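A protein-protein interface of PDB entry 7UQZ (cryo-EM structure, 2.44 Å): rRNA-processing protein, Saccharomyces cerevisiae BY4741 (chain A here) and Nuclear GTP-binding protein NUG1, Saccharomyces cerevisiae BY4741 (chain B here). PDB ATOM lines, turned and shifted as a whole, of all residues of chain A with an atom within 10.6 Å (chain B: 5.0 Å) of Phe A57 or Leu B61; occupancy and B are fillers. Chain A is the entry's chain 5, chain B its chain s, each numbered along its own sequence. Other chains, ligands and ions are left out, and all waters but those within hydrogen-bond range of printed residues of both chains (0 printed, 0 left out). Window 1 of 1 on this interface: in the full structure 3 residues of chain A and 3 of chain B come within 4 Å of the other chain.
The side-chain amino group (NZ) of Lys B57 lies within salt-bridge range of the side-chain carboxylate (OD1) of Asp A54 (3.0 Å).
CE1 of Phe A57 touches O of Lys B57, 3.4 Å away. Phe A57 touches Leu B61. CD1 of Leu A64 touches CD1 of Leu B61, at 3.8 Å. Leu A64 touches Glu B65.
Of the printed residues of chain B, Asp A54 touches Lys B57 (3.0 Å). Of chain B, only Lys B57 and Leu B61 come within 4 Å of Phe A57. Printed residues of chain B within 4 Å of Leu A64: Leu B61 (3.8 Å) and Glu B65 (3.3 Å). Ile B50 touches none of the printed residues of chain A. Of chain A, only Asp A54 (3.0 Å) and Phe A57 (3.4 Å) come within 4 Å of Lys B57. No residue of chain A comes within 4 Å of Ala B58. Of chain A, only Phe A57 (3.7 Å) and Leu A64 (3.8 Å) come within 4 Å of Leu B61. Glu B62 touches none of the printed residues of chain A. Glu B63 touches none of the printed residues of chain A. Of chain A, only Leu A64 (3.3 Å) comes within 4 Å of Glu B65. The nearest residue of chain A that does not touch Leu B61 is Arg A60 (4.5 Å).
Of the 11 printed residues of chain B, 3 touch a printed residue of chain A. Printed residues of chain B that touch a printed residue of chain A: Lys B57, Leu B61 and Glu B65. Hydrophobic or aromatic side chains of chain B within 4 Å of the printed part of chain A: Leu B61. Among the printed residues, 5 pairs touch across the chains. Among the printed residues, Asp or Glu carboxylates within 4 Å of a Lys or Arg side-chain nitrogen of the other chain: Asp A54 with Lys B57.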
ATOM      1  N   GLN A  49     -33.261 -22.489 -24.193  1.00  0.00           N
ATOM      2  CA  GLN A  49     -33.939 -22.572 -22.903  1.00  0.00           C
ATOM      3  C   GLN A  49     -32.952 -22.854 -21.776  1.00  0.00           C
ATOM      4  O   GLN A  49     -33.075 -22.296 -20.677  1.00  0.00           O
ATOM      5  CB  GLN A  49     -35.024 -23.648 -22.950  1.00  0.00           C
ATOM      6  CG  GLN A  49     -35.943 -23.648 -21.741  1.00  0.00           C
ATOM      7  CD  GLN A  49     -36.747 -22.368 -21.623  1.00  0.00           C
ATOM      8  OE1 GLN A  49     -37.188 -21.804 -22.625  1.00  0.00           O
ATOM      9  NE2 GLN A  49     -36.936 -21.898 -20.397  1.00  0.00           N
ATOM     10  N   LYS A  50     -31.966 -23.719 -22.031  1.00  0.00           N
ATOM     11  CA  LYS A  50     -30.918 -23.963 -21.045  1.00  0.00           C
ATOM     12  C   LYS A  50     -30.119 -22.695 -20.765  1.00  0.00           C
ATOM     13  O   LYS A  50     -29.779 -22.409 -19.610  1.00  0.00           O
ATOM     14  CB  LYS A  50     -29.994 -25.084 -21.523  1.00  0.00           C
ATOM     15  CG  LYS A  50     -30.630 -26.467 -21.518  1.00  0.00           C
ATOM     16  CD  LYS A  50     -31.030 -26.891 -20.115  1.00  0.00           C
ATOM     17  CE  LYS A  50     -31.640 -28.283 -20.111  1.00  0.00           C
ATOM     18  NZ  LYS A  50     -32.891 -28.352 -20.917  1.00  0.00           N
ATOM     19  N   ARG A  51     -29.818 -21.921 -21.813  1.00  0.00           N
ATOM     20  CA  ARG A  51     -29.115 -20.653 -21.632  1.00  0.00           C
ATOM     21  C   ARG A  51     -29.924 -19.691 -20.768  1.00  0.00           C
ATOM     22  O   ARG A  51     -29.383 -19.041 -19.864  1.00  0.00           O
ATOM     23  CB  ARG A  51     -28.818 -20.021 -22.993  1.00  0.00           C
ATOM     24  CG  ARG A  51     -27.728 -20.709 -23.791  1.00  0.00           C
ATOM     25  CD  ARG A  51     -27.316 -19.856 -24.980  1.00  0.00           C
ATOM     26  NE  ARG A  51     -28.195 -20.024 -26.129  1.00  0.00           N
ATOM     27  CZ  ARG A  51     -28.245 -19.190 -27.160  1.00  0.00           C
ATOM     28  NH1 ARG A  51     -27.516 -18.087 -27.192  1.00  0.00           N
ATOM     29  NH2 ARG A  51     -29.051 -19.467 -28.180  1.00  0.00           N
ATOM     30  N   LEU A  52     -31.230 -19.595 -21.034  1.00  0.00           N
ATOM     31  CA  LEU A  52     -32.084 -18.689 -20.267  1.00  0.00           C
ATOM     32  C   LEU A  52     -32.179 -19.114 -18.805  1.00  0.00           C
ATOM     33  O   LEU A  52     -32.120 -18.271 -17.896  1.00  0.00           O
ATOM     34  CB  LEU A  52     -33.473 -18.625 -20.900  1.00  0.00           C
ATOM     35  CG  LEU A  52     -34.480 -17.679 -20.245  1.00  0.00           C
ATOM     36  CD1 LEU A  52     -34.012 -16.238 -20.354  1.00  0.00           C
ATOM     37  CD2 LEU A  52     -35.858 -17.851 -20.865  1.00  0.00           C
ATOM     38  N   GLU A  53     -32.323 -20.418 -18.554  1.00  0.00           N
ATOM     39  CA  GLU A  53     -32.383 -20.905 -17.178  1.00  0.00           C
ATOM     40  C   GLU A  53     -31.066 -20.673 -16.447  1.00  0.00           C
ATOM     41  O   GLU A  53     -31.061 -20.321 -15.259  1.00  0.00           O
ATOM     42  CB  GLU A  53     -32.763 -22.384 -17.162  1.00  0.00           C
ATOM     43  CG  GLU A  53     -34.218 -22.642 -17.513  1.00  0.00           C
ATOM     44  CD  GLU A  53     -34.570 -24.113 -17.508  1.00  0.00           C
ATOM     45  OE1 GLU A  53     -33.804 -24.912 -18.087  1.00  0.00           O
ATOM     46  OE2 GLU A  53     -35.610 -24.474 -16.919  1.00  0.00           O
ATOM     47  N   ASP A  54     -29.937 -20.866 -17.137  1.00  0.00           N
ATOM     48  CA  ASP A  54     -28.641 -20.593 -16.525  1.00  0.00           C
ATOM     49  C   ASP A  54     -28.491 -19.115 -16.186  1.00  0.00           C
ATOM     50  O   ASP A  54     -27.958 -18.767 -15.125  1.00  0.00           O
ATOM     51  CB  ASP A  54     -27.513 -21.047 -17.449  1.00  0.00           C
ATOM     52  CG  ASP A  54     -26.162 -21.042 -16.762  1.00  0.00           C
ATOM     53  OD1 ASP A  54     -25.869 -21.997 -16.013  1.00  0.00           O
ATOM     54  OD2 ASP A  54     -25.393 -20.081 -16.968  1.00  0.00           O
ATOM     55  N   LYS A  55     -28.953 -18.231 -17.077  1.00  0.00           N
ATOM     56  CA  LYS A  55     -28.904 -16.799 -16.786  1.00  0.00           C
ATOM     57  C   LYS A  55     -29.764 -16.448 -15.576  1.00  0.00           C
ATOM     58  O   LYS A  55     -29.363 -15.628 -14.739  1.00  0.00           O
ATOM     59  CB  LYS A  55     -29.350 -15.992 -18.005  1.00  0.00           C
ATOM     60  CG  LYS A  55     -28.334 -15.940 -19.134  1.00  0.00           C
ATOM     61  CD  LYS A  55     -28.754 -14.944 -20.203  1.00  0.00           C
ATOM     62  CE  LYS A  55     -27.671 -14.770 -21.258  1.00  0.00           C
ATOM     63  NZ  LYS A  55     -27.382 -16.038 -21.981  1.00  0.00           N
ATOM     64  N   GLN A  56     -30.952 -17.054 -15.470  1.00  0.00           N
ATOM     65  CA  GLN A  56     -31.804 -16.803 -14.310  1.00  0.00           C
ATOM     66  C   GLN A  56     -31.139 -17.270 -13.018  1.00  0.00           C
ATOM     67  O   GLN A  56     -31.175 -16.565 -11.999  1.00  0.00           O
ATOM     68  CB  GLN A  56     -33.162 -17.483 -14.486  1.00  0.00           C
ATOM     69  CG  GLN A  56     -34.075 -16.806 -15.491  1.00  0.00           C
ATOM     70  CD  GLN A  56     -35.538 -17.094 -15.230  1.00  0.00           C
ATOM     71  OE1 GLN A  56     -35.899 -17.648 -14.191  1.00  0.00           O
ATOM     72  NE2 GLN A  56     -36.393 -16.718 -16.174  1.00  0.00           N
ATOM     73  N   PHE A  57     -30.520 -18.454 -13.045  1.00  0.00           N
ATOM     74  CA  PHE A  57     -29.814 -18.939 -11.862  1.00  0.00           C
ATOM     75  C   PHE A  57     -28.664 -18.013 -11.485  1.00  0.00           C
ATOM     76  O   PHE A  57     -28.465 -17.706 -10.302  1.00  0.00           O
ATOM     77  CB  PHE A  57     -29.295 -20.358 -12.094  1.00  0.00           C
ATOM     78  CG  PHE A  57     -28.418 -20.870 -10.984  1.00  0.00           C
ATOM     79  CD1 PHE A  57     -28.974 -21.338  -9.804  1.00  0.00           C
ATOM     80  CD2 PHE A  57     -27.040 -20.882 -11.117  1.00  0.00           C
ATOM     81  CE1 PHE A  57     -28.171 -21.808  -8.779  1.00  0.00           C
ATOM     82  CE2 PHE A  57     -26.233 -21.349 -10.093  1.00  0.00           C
ATOM     83  CZ  PHE A  57     -26.800 -21.812  -8.926  1.00  0.00           C
ATOM     84  N   LYS A  58     -27.897 -17.559 -12.481  1.00  0.00           N
ATOM     85  CA  LYS A  58     -26.756 -16.692 -12.204  1.00  0.00           C
ATOM     86  C   LYS A  58     -27.199 -15.357 -11.621  1.00  0.00           C
ATOM     87  O   LYS A  58     -26.572 -14.847 -10.685  1.00  0.00           O
ATOM     88  CB  LYS A  58     -25.935 -16.478 -13.475  1.00  0.00           C
ATOM     89  CG  LYS A  58     -25.154 -17.703 -13.927  1.00  0.00           C
ATOM     90  CD  LYS A  58     -24.388 -17.430 -15.209  1.00  0.00           C
ATOM     91  CE  LYS A  58     -23.218 -16.487 -14.968  1.00  0.00           C
ATOM     92  NZ  LYS A  58     -22.162 -17.121 -14.132  1.00  0.00           N
ATOM     93  N   GLU A  59     -28.281 -14.776 -12.149  1.00  0.00           N
ATOM     94  CA  GLU A  59     -28.722 -13.485 -11.628  1.00  0.00           C
ATOM     95  C   GLU A  59     -29.319 -13.624 -10.230  1.00  0.00           C
ATOM     96  O   GLU A  59     -29.121 -12.744  -9.382  1.00  0.00           O
ATOM     97  CB  GLU A  59     -29.705 -12.814 -12.593  1.00  0.00           C
ATOM     98  CG  GLU A  59     -31.030 -13.519 -12.789  1.00  0.00           C
ATOM     99  CD  GLU A  59     -31.907 -12.839 -13.819  1.00  0.00           C
ATOM    100  OE1 GLU A  59     -31.482 -11.804 -14.375  1.00  0.00           O
ATOM    101  OE2 GLU A  59     -33.023 -13.341 -14.073  1.00  0.00           O
ATOM    102  N   ARG A  60     -30.020 -14.732  -9.952  1.00  0.00           N
ATOM    103  CA  ARG A  60     -30.516 -14.954  -8.595  1.00  0.00           C
ATOM    104  C   ARG A  60     -29.370 -15.129  -7.602  1.00  0.00           C
ATOM    105  O   ARG A  60     -29.397 -14.561  -6.499  1.00  0.00           O
ATOM    106  CB  ARG A  60     -31.442 -16.171  -8.563  1.00  0.00           C
ATOM    107  CG  ARG A  60     -32.722 -16.017  -9.386  1.00  0.00           C
ATOM    108  CD  ARG A  60     -33.742 -15.088  -8.725  1.00  0.00           C
ATOM    109  NE  ARG A  60     -34.289 -15.629  -7.486  1.00  0.00           N
ATOM    110  CZ  ARG A  60     -35.071 -14.955  -6.653  1.00  0.00           C
ATOM    111  NH1 ARG A  60     -35.433 -13.707  -6.901  1.00  0.00           N
ATOM    112  NH2 ARG A  60     -35.501 -15.549  -5.542  1.00  0.00           N
ATOM    113  N   LEU A  61     -28.349 -15.906  -7.981  1.00  0.00           N
ATOM    114  CA  LEU A  61     -27.192 -16.089  -7.111  1.00  0.00           C
ATOM    115  C   LEU A  61     -26.452 -14.775  -6.889  1.00  0.00           C
ATOM    116  O   LEU A  61     -26.003 -14.488  -5.773  1.00  0.00           O
ATOM    117  CB  LEU A  61     -26.255 -17.143  -7.703  1.00  0.00           C
ATOM    118  CG  LEU A  61     -25.051 -17.539  -6.850  1.00  0.00           C
ATOM    119  CD1 LEU A  61     -25.504 -18.161  -5.538  1.00  0.00           C
ATOM    120  CD2 LEU A  61     -24.142 -18.487  -7.612  1.00  0.00           C
ATOM    121  N   LYS A  62     -26.317 -13.964  -7.944  1.00  0.00           N
ATOM    122  CA  LYS A  62     -25.665 -12.666  -7.811  1.00  0.00           C
ATOM    123  C   LYS A  62     -26.445 -11.746  -6.881  1.00  0.00           C
ATOM    124  O   LYS A  62     -25.850 -11.027  -6.071  1.00  0.00           O
ATOM    125  CB  LYS A  62     -25.496 -12.022  -9.188  1.00  0.00           C
ATOM    126  CG  LYS A  62     -24.872 -10.633  -9.160  1.00  0.00           C
ATOM    127  CD  LYS A  62     -24.632 -10.106 -10.568  1.00  0.00           C
ATOM    128  CE  LYS A  62     -24.107  -8.680 -10.549  1.00  0.00           C
ATOM    129  NZ  LYS A  62     -25.107  -7.727  -9.991  1.00  0.00           N
ATOM    130  N   ALA A  63     -27.778 -11.756  -6.979  1.00  0.00           N
ATOM    131  CA  ALA A  63     -28.592 -10.941  -6.080  1.00  0.00           C
ATOM    132  C   ALA A  63     -28.424 -11.377  -4.629  1.00  0.00           C
ATOM    133  O   ALA A  63     -28.286 -10.533  -3.732  1.00  0.00           O
ATOM    134  CB  ALA A  63     -30.062 -11.014  -6.494  1.00  0.00           C
ATOM    135  N   LEU A  64     -28.423 -12.692  -4.383  1.00  0.00           N
ATOM    136  CA  LEU A  64     -28.228 -13.188  -3.021  1.00  0.00           C
ATOM    137  C   LEU A  64     -26.858 -12.799  -2.477  1.00  0.00           C
ATOM    138  O   LEU A  64     -26.739 -12.351  -1.327  1.00  0.00           O
ATOM    139  CB  LEU A  64     -28.402 -14.705  -2.982  1.00  0.00           C
ATOM    140  CG  LEU A  64     -29.815 -15.260  -3.160  1.00  0.00           C
ATOM    141  CD1 LEU A  64     -29.787 -16.776  -3.125  1.00  0.00           C
ATOM    142  CD2 LEU A  64     -30.737 -14.716  -2.085  1.00  0.00           C
ATOM    143  N   LYS A  65     -25.811 -12.958  -3.292  1.00  0.00           N
ATOM    144  CA  LYS A  65     -24.468 -12.594  -2.852  1.00  0.00           C
ATOM    145  C   LYS A  65     -24.363 -11.099  -2.576  1.00  0.00           C
ATOM    146  O   LYS A  65     -23.737 -10.686  -1.591  1.00  0.00           O
ATOM    147  CB  LYS A  65     -23.440 -13.022  -3.898  1.00  0.00           C
ATOM    148  CG  LYS A  65     -23.236 -14.526  -3.991  1.00  0.00           C
ATOM    149  CD  LYS A  65     -22.275 -14.886  -5.112  1.00  0.00           C
ATOM    150  CE  LYS A  65     -21.975 -16.375  -5.127  1.00  0.00           C
ATOM    151  NZ  LYS A  65     -21.363 -16.834  -3.850  1.00  0.00           N
ATOM    152  N   GLU A  67     -26.807  -8.958  -1.689  1.00  0.00           N
ATOM    153  CA  GLU A  67     -27.502  -8.562  -0.466  1.00  0.00           C
ATOM    154  C   GLU A  67     -26.770  -9.066   0.776  1.00  0.00           C
ATOM    155  O   GLU A  67     -26.730  -8.371   1.801  1.00  0.00           O
ATOM    156  CB  GLU A  67     -28.961  -9.034  -0.486  1.00  0.00           C
ATOM    157  CG  GLU A  67     -29.190 -10.527  -0.615  1.00  0.00           C
ATOM    158  CD  GLU A  67     -29.212 -11.249   0.720  1.00  0.00           C
ATOM    159  OE1 GLU A  67     -29.280 -10.573   1.767  1.00  0.00           O
ATOM    160  OE2 GLU A  67     -29.159 -12.497   0.722  1.00  0.00           O
ATOM    161  N   LYS A  68     -26.160 -10.256   0.701  1.00  0.00           N
ATOM    162  CA  LYS A  68     -25.386 -10.751   1.837  1.00  0.00           C
ATOM    163  C   LYS A  68     -24.169  -9.870   2.105  1.00  0.00           C
ATOM    164  O   LYS A  68     -23.880  -9.527   3.262  1.00  0.00           O
ATOM    165  CB  LYS A  68     -24.965 -12.199   1.587  1.00  0.00           C
ATOM    166  CG  LYS A  68     -24.568 -12.962   2.839  1.00  0.00           C
ATOM    167  CD  LYS A  68     -24.486 -14.457   2.565  1.00  0.00           C
ATOM    168  CE  LYS A  68     -24.284 -15.248   3.847  1.00  0.00           C
ATOM    169  NZ  LYS A  68     -23.025 -14.872   4.550  1.00  0.00           N
ATOM    170  N   ILE B  50     -21.515 -24.074  -5.330  1.00  0.00           N
ATOM    171  CA  ILE B  50     -22.073 -24.984  -6.327  1.00  0.00           C
ATOM    172  C   ILE B  50     -21.315 -24.839  -7.641  1.00  0.00           C
ATOM    173  O   ILE B  50     -21.163 -23.717  -8.146  1.00  0.00           O
ATOM    174  CB  ILE B  50     -23.573 -24.723  -6.531  1.00  0.00           C
ATOM    175  CG1 ILE B  50     -24.261 -24.485  -5.186  1.00  0.00           C
ATOM    176  CG2 ILE B  50     -24.222 -25.891  -7.251  1.00  0.00           C
ATOM    177  CD1 ILE B  50     -25.649 -23.898  -5.308  1.00  0.00           C
ATOM    178  N   LYS B  57     -28.535 -27.243  -9.965  1.00  0.00           N
ATOM    179  CA  LYS B  57     -28.150 -26.052  -9.216  1.00  0.00           C
ATOM    180  C   LYS B  57     -29.373 -25.319  -8.689  1.00  0.00           C
ATOM    181  O   LYS B  57     -29.362 -24.806  -7.563  1.00  0.00           O
ATOM    182  CB  LYS B  57     -27.325 -25.115 -10.094  1.00  0.00           C
ATOM    183  CG  LYS B  57     -25.976 -25.645 -10.508  1.00  0.00           C
ATOM    184  CD  LYS B  57     -25.224 -24.606 -11.324  1.00  0.00           C
ATOM    185  CE  LYS B  57     -26.044 -24.127 -12.509  1.00  0.00           C
ATOM    186  NZ  LYS B  57     -25.271 -23.187 -13.365  1.00  0.00           N
ATOM    187  N   ALA B  58     -30.432 -25.243  -9.499  1.00  0.00           N
ATOM    188  CA  ALA B  58     -31.660 -24.591  -9.061  1.00  0.00           C
ATOM    189  C   ALA B  58     -32.275 -25.322  -7.878  1.00  0.00           C
ATOM    190  O   ALA B  58     -32.752 -24.689  -6.930  1.00  0.00           O
ATOM    191  CB  ALA B  58     -32.654 -24.504 -10.216  1.00  0.00           C
ATOM    192  N   LYS B  59     -32.267 -26.656  -7.911  1.00  0.00           N
ATOM    193  CA  LYS B  59     -32.800 -27.430  -6.794  1.00  0.00           C
ATOM    194  C   LYS B  59     -31.980 -27.211  -5.529  1.00  0.00           C
ATOM    195  O   LYS B  59     -32.544 -27.045  -4.440  1.00  0.00           O
ATOM    196  CB  LYS B  59     -32.847 -28.913  -7.156  1.00  0.00           C
ATOM    197  CG  LYS B  59     -33.809 -29.245  -8.283  1.00  0.00           C
ATOM    198  CD  LYS B  59     -33.865 -30.743  -8.537  1.00  0.00           C
ATOM    199  CE  LYS B  59     -34.904 -31.081  -9.595  1.00  0.00           C
ATOM    200  NZ  LYS B  59     -34.651 -30.363 -10.874  1.00  0.00           N
ATOM    201  N   ILE B  60     -30.648 -27.195  -5.653  1.00  0.00           N
ATOM    202  CA  ILE B  60     -29.800 -26.954  -4.485  1.00  0.00           C
ATOM    203  C   ILE B  60     -30.050 -25.560  -3.912  1.00  0.00           C
ATOM    204  O   ILE B  60     -30.151 -25.383  -2.690  1.00  0.00           O
ATOM    205  CB  ILE B  60     -28.317 -27.163  -4.850  1.00  0.00           C
ATOM    206  CG1 ILE B  60     -28.056 -28.625  -5.209  1.00  0.00           C
ATOM    207  CG2 ILE B  60     -27.412 -26.747  -3.702  1.00  0.00           C
ATOM    208  CD1 ILE B  60     -28.348 -29.588  -4.085  1.00  0.00           C
ATOM    209  N   LEU B  61     -30.163 -24.554  -4.784  1.00  0.00           N
ATOM    210  CA  LEU B  61     -30.389 -23.187  -4.322  1.00  0.00           C
ATOM    211  C   LEU B  61     -31.760 -23.034  -3.669  1.00  0.00           C
ATOM    212  O   LEU B  61     -31.893 -22.350  -2.647  1.00  0.00           O
ATOM    213  CB  LEU B  61     -30.232 -22.210  -5.487  1.00  0.00           C
ATOM    214  CG  LEU B  61     -30.293 -20.721  -5.147  1.00  0.00           C
ATOM    215  CD1 LEU B  61     -29.200 -20.353  -4.157  1.00  0.00           C
ATOM    216  CD2 LEU B  61     -30.186 -19.879  -6.410  1.00  0.00           C
ATOM    217  N   GLU B  62     -32.789 -23.664  -4.242  1.00  0.00           N
ATOM    218  CA  GLU B  62     -34.115 -23.622  -3.633  1.00  0.00           C
ATOM    219  C   GLU B  62     -34.116 -24.305  -2.273  1.00  0.00           C
ATOM    220  O   GLU B  62     -34.740 -23.813  -1.325  1.00  0.00           O
ATOM    221  CB  GLU B  62     -35.143 -24.276  -4.558  1.00  0.00           C
ATOM    222  CG  GLU B  62     -35.491 -23.457  -5.788  1.00  0.00           C
ATOM    223  CD  GLU B  62     -36.284 -24.254  -6.805  1.00  0.00           C
ATOM    224  OE1 GLU B  62     -36.666 -25.400  -6.492  1.00  0.00           O
ATOM    225  OE2 GLU B  62     -36.520 -23.739  -7.918  1.00  0.00           O
ATOM    226  N   GLU B  63     -33.417 -25.438  -2.155  1.00  0.00           N
ATOM    227  CA  GLU B  63     -33.347 -26.125  -0.871  1.00  0.00           C
ATOM    228  C   GLU B  63     -32.629 -25.281   0.173  1.00  0.00           C
ATOM    229  O   GLU B  63     -33.070 -25.213   1.326  1.00  0.00           O
ATOM    230  CB  GLU B  63     -32.661 -27.482  -1.029  1.00  0.00           C
ATOM    231  CG  GLU B  63     -33.520 -28.539  -1.704  1.00  0.00           C
ATOM    232  CD  GLU B  63     -32.918 -29.925  -1.606  1.00  0.00           C
ATOM    233  OE1 GLU B  63     -32.175 -30.186  -0.636  1.00  0.00           O
ATOM    234  OE2 GLU B  63     -33.185 -30.755  -2.500  1.00  0.00           O
ATOM    235  N   ILE B  64     -31.526 -24.625  -0.202  1.00  0.00           N
ATOM    236  CA  ILE B  64     -30.812 -23.830   0.794  1.00  0.00           C
ATOM    237  C   ILE B  64     -31.608 -22.577   1.162  1.00  0.00           C
ATOM    238  O   ILE B  64     -31.577 -22.136   2.319  1.00  0.00           O
ATOM    239  CB  ILE B  64     -29.374 -23.507   0.329  1.00  0.00           C
ATOM    240  CG1 ILE B  64     -28.526 -23.041   1.514  1.00  0.00           C
ATOM    241  CG2 ILE B  64     -29.343 -22.458  -0.767  1.00  0.00           C
ATOM    242  CD1 ILE B  64     -28.492 -24.022   2.667  1.00  0.00           C
ATOM    243  N   GLU B  65     -32.364 -22.007   0.216  1.00  0.00           N
ATOM    244  CA  GLU B  65     -33.241 -20.889   0.553  1.00  0.00           C
ATOM    245  C   GLU B  65     -34.355 -21.321   1.500  1.00  0.00           C
ATOM    246  O   GLU B  65     -34.694 -20.591   2.439  1.00  0.00           O
ATOM    247  CB  GLU B  65     -33.830 -20.274  -0.715  1.00  0.00           C
ATOM    248  CG  GLU B  65     -32.867 -19.393  -1.490  1.00  0.00           C
ATOM    249  CD  GLU B  65     -33.485 -18.843  -2.758  1.00  0.00           C
ATOM    250  OE1 GLU B  65     -34.592 -19.293  -3.120  1.00  0.00           O
ATOM    251  OE2 GLU B  65     -32.868 -17.961  -3.391  1.00  0.00           O
ATOM    252  N   ALA B  66     -34.938 -22.501   1.267  1.00  0.00           N
ATOM    253  CA  ALA B  66     -35.972 -23.007   2.164  1.00  0.00           C
ATOM    254  C   ALA B  66     -35.411 -23.288   3.552  1.00  0.00           C
ATOM    255  O   ALA B  66     -36.067 -23.010   4.564  1.00  0.00           O
ATOM    256  CB  ALA B  66     -36.607 -24.266   1.576  1.00  0.00           C
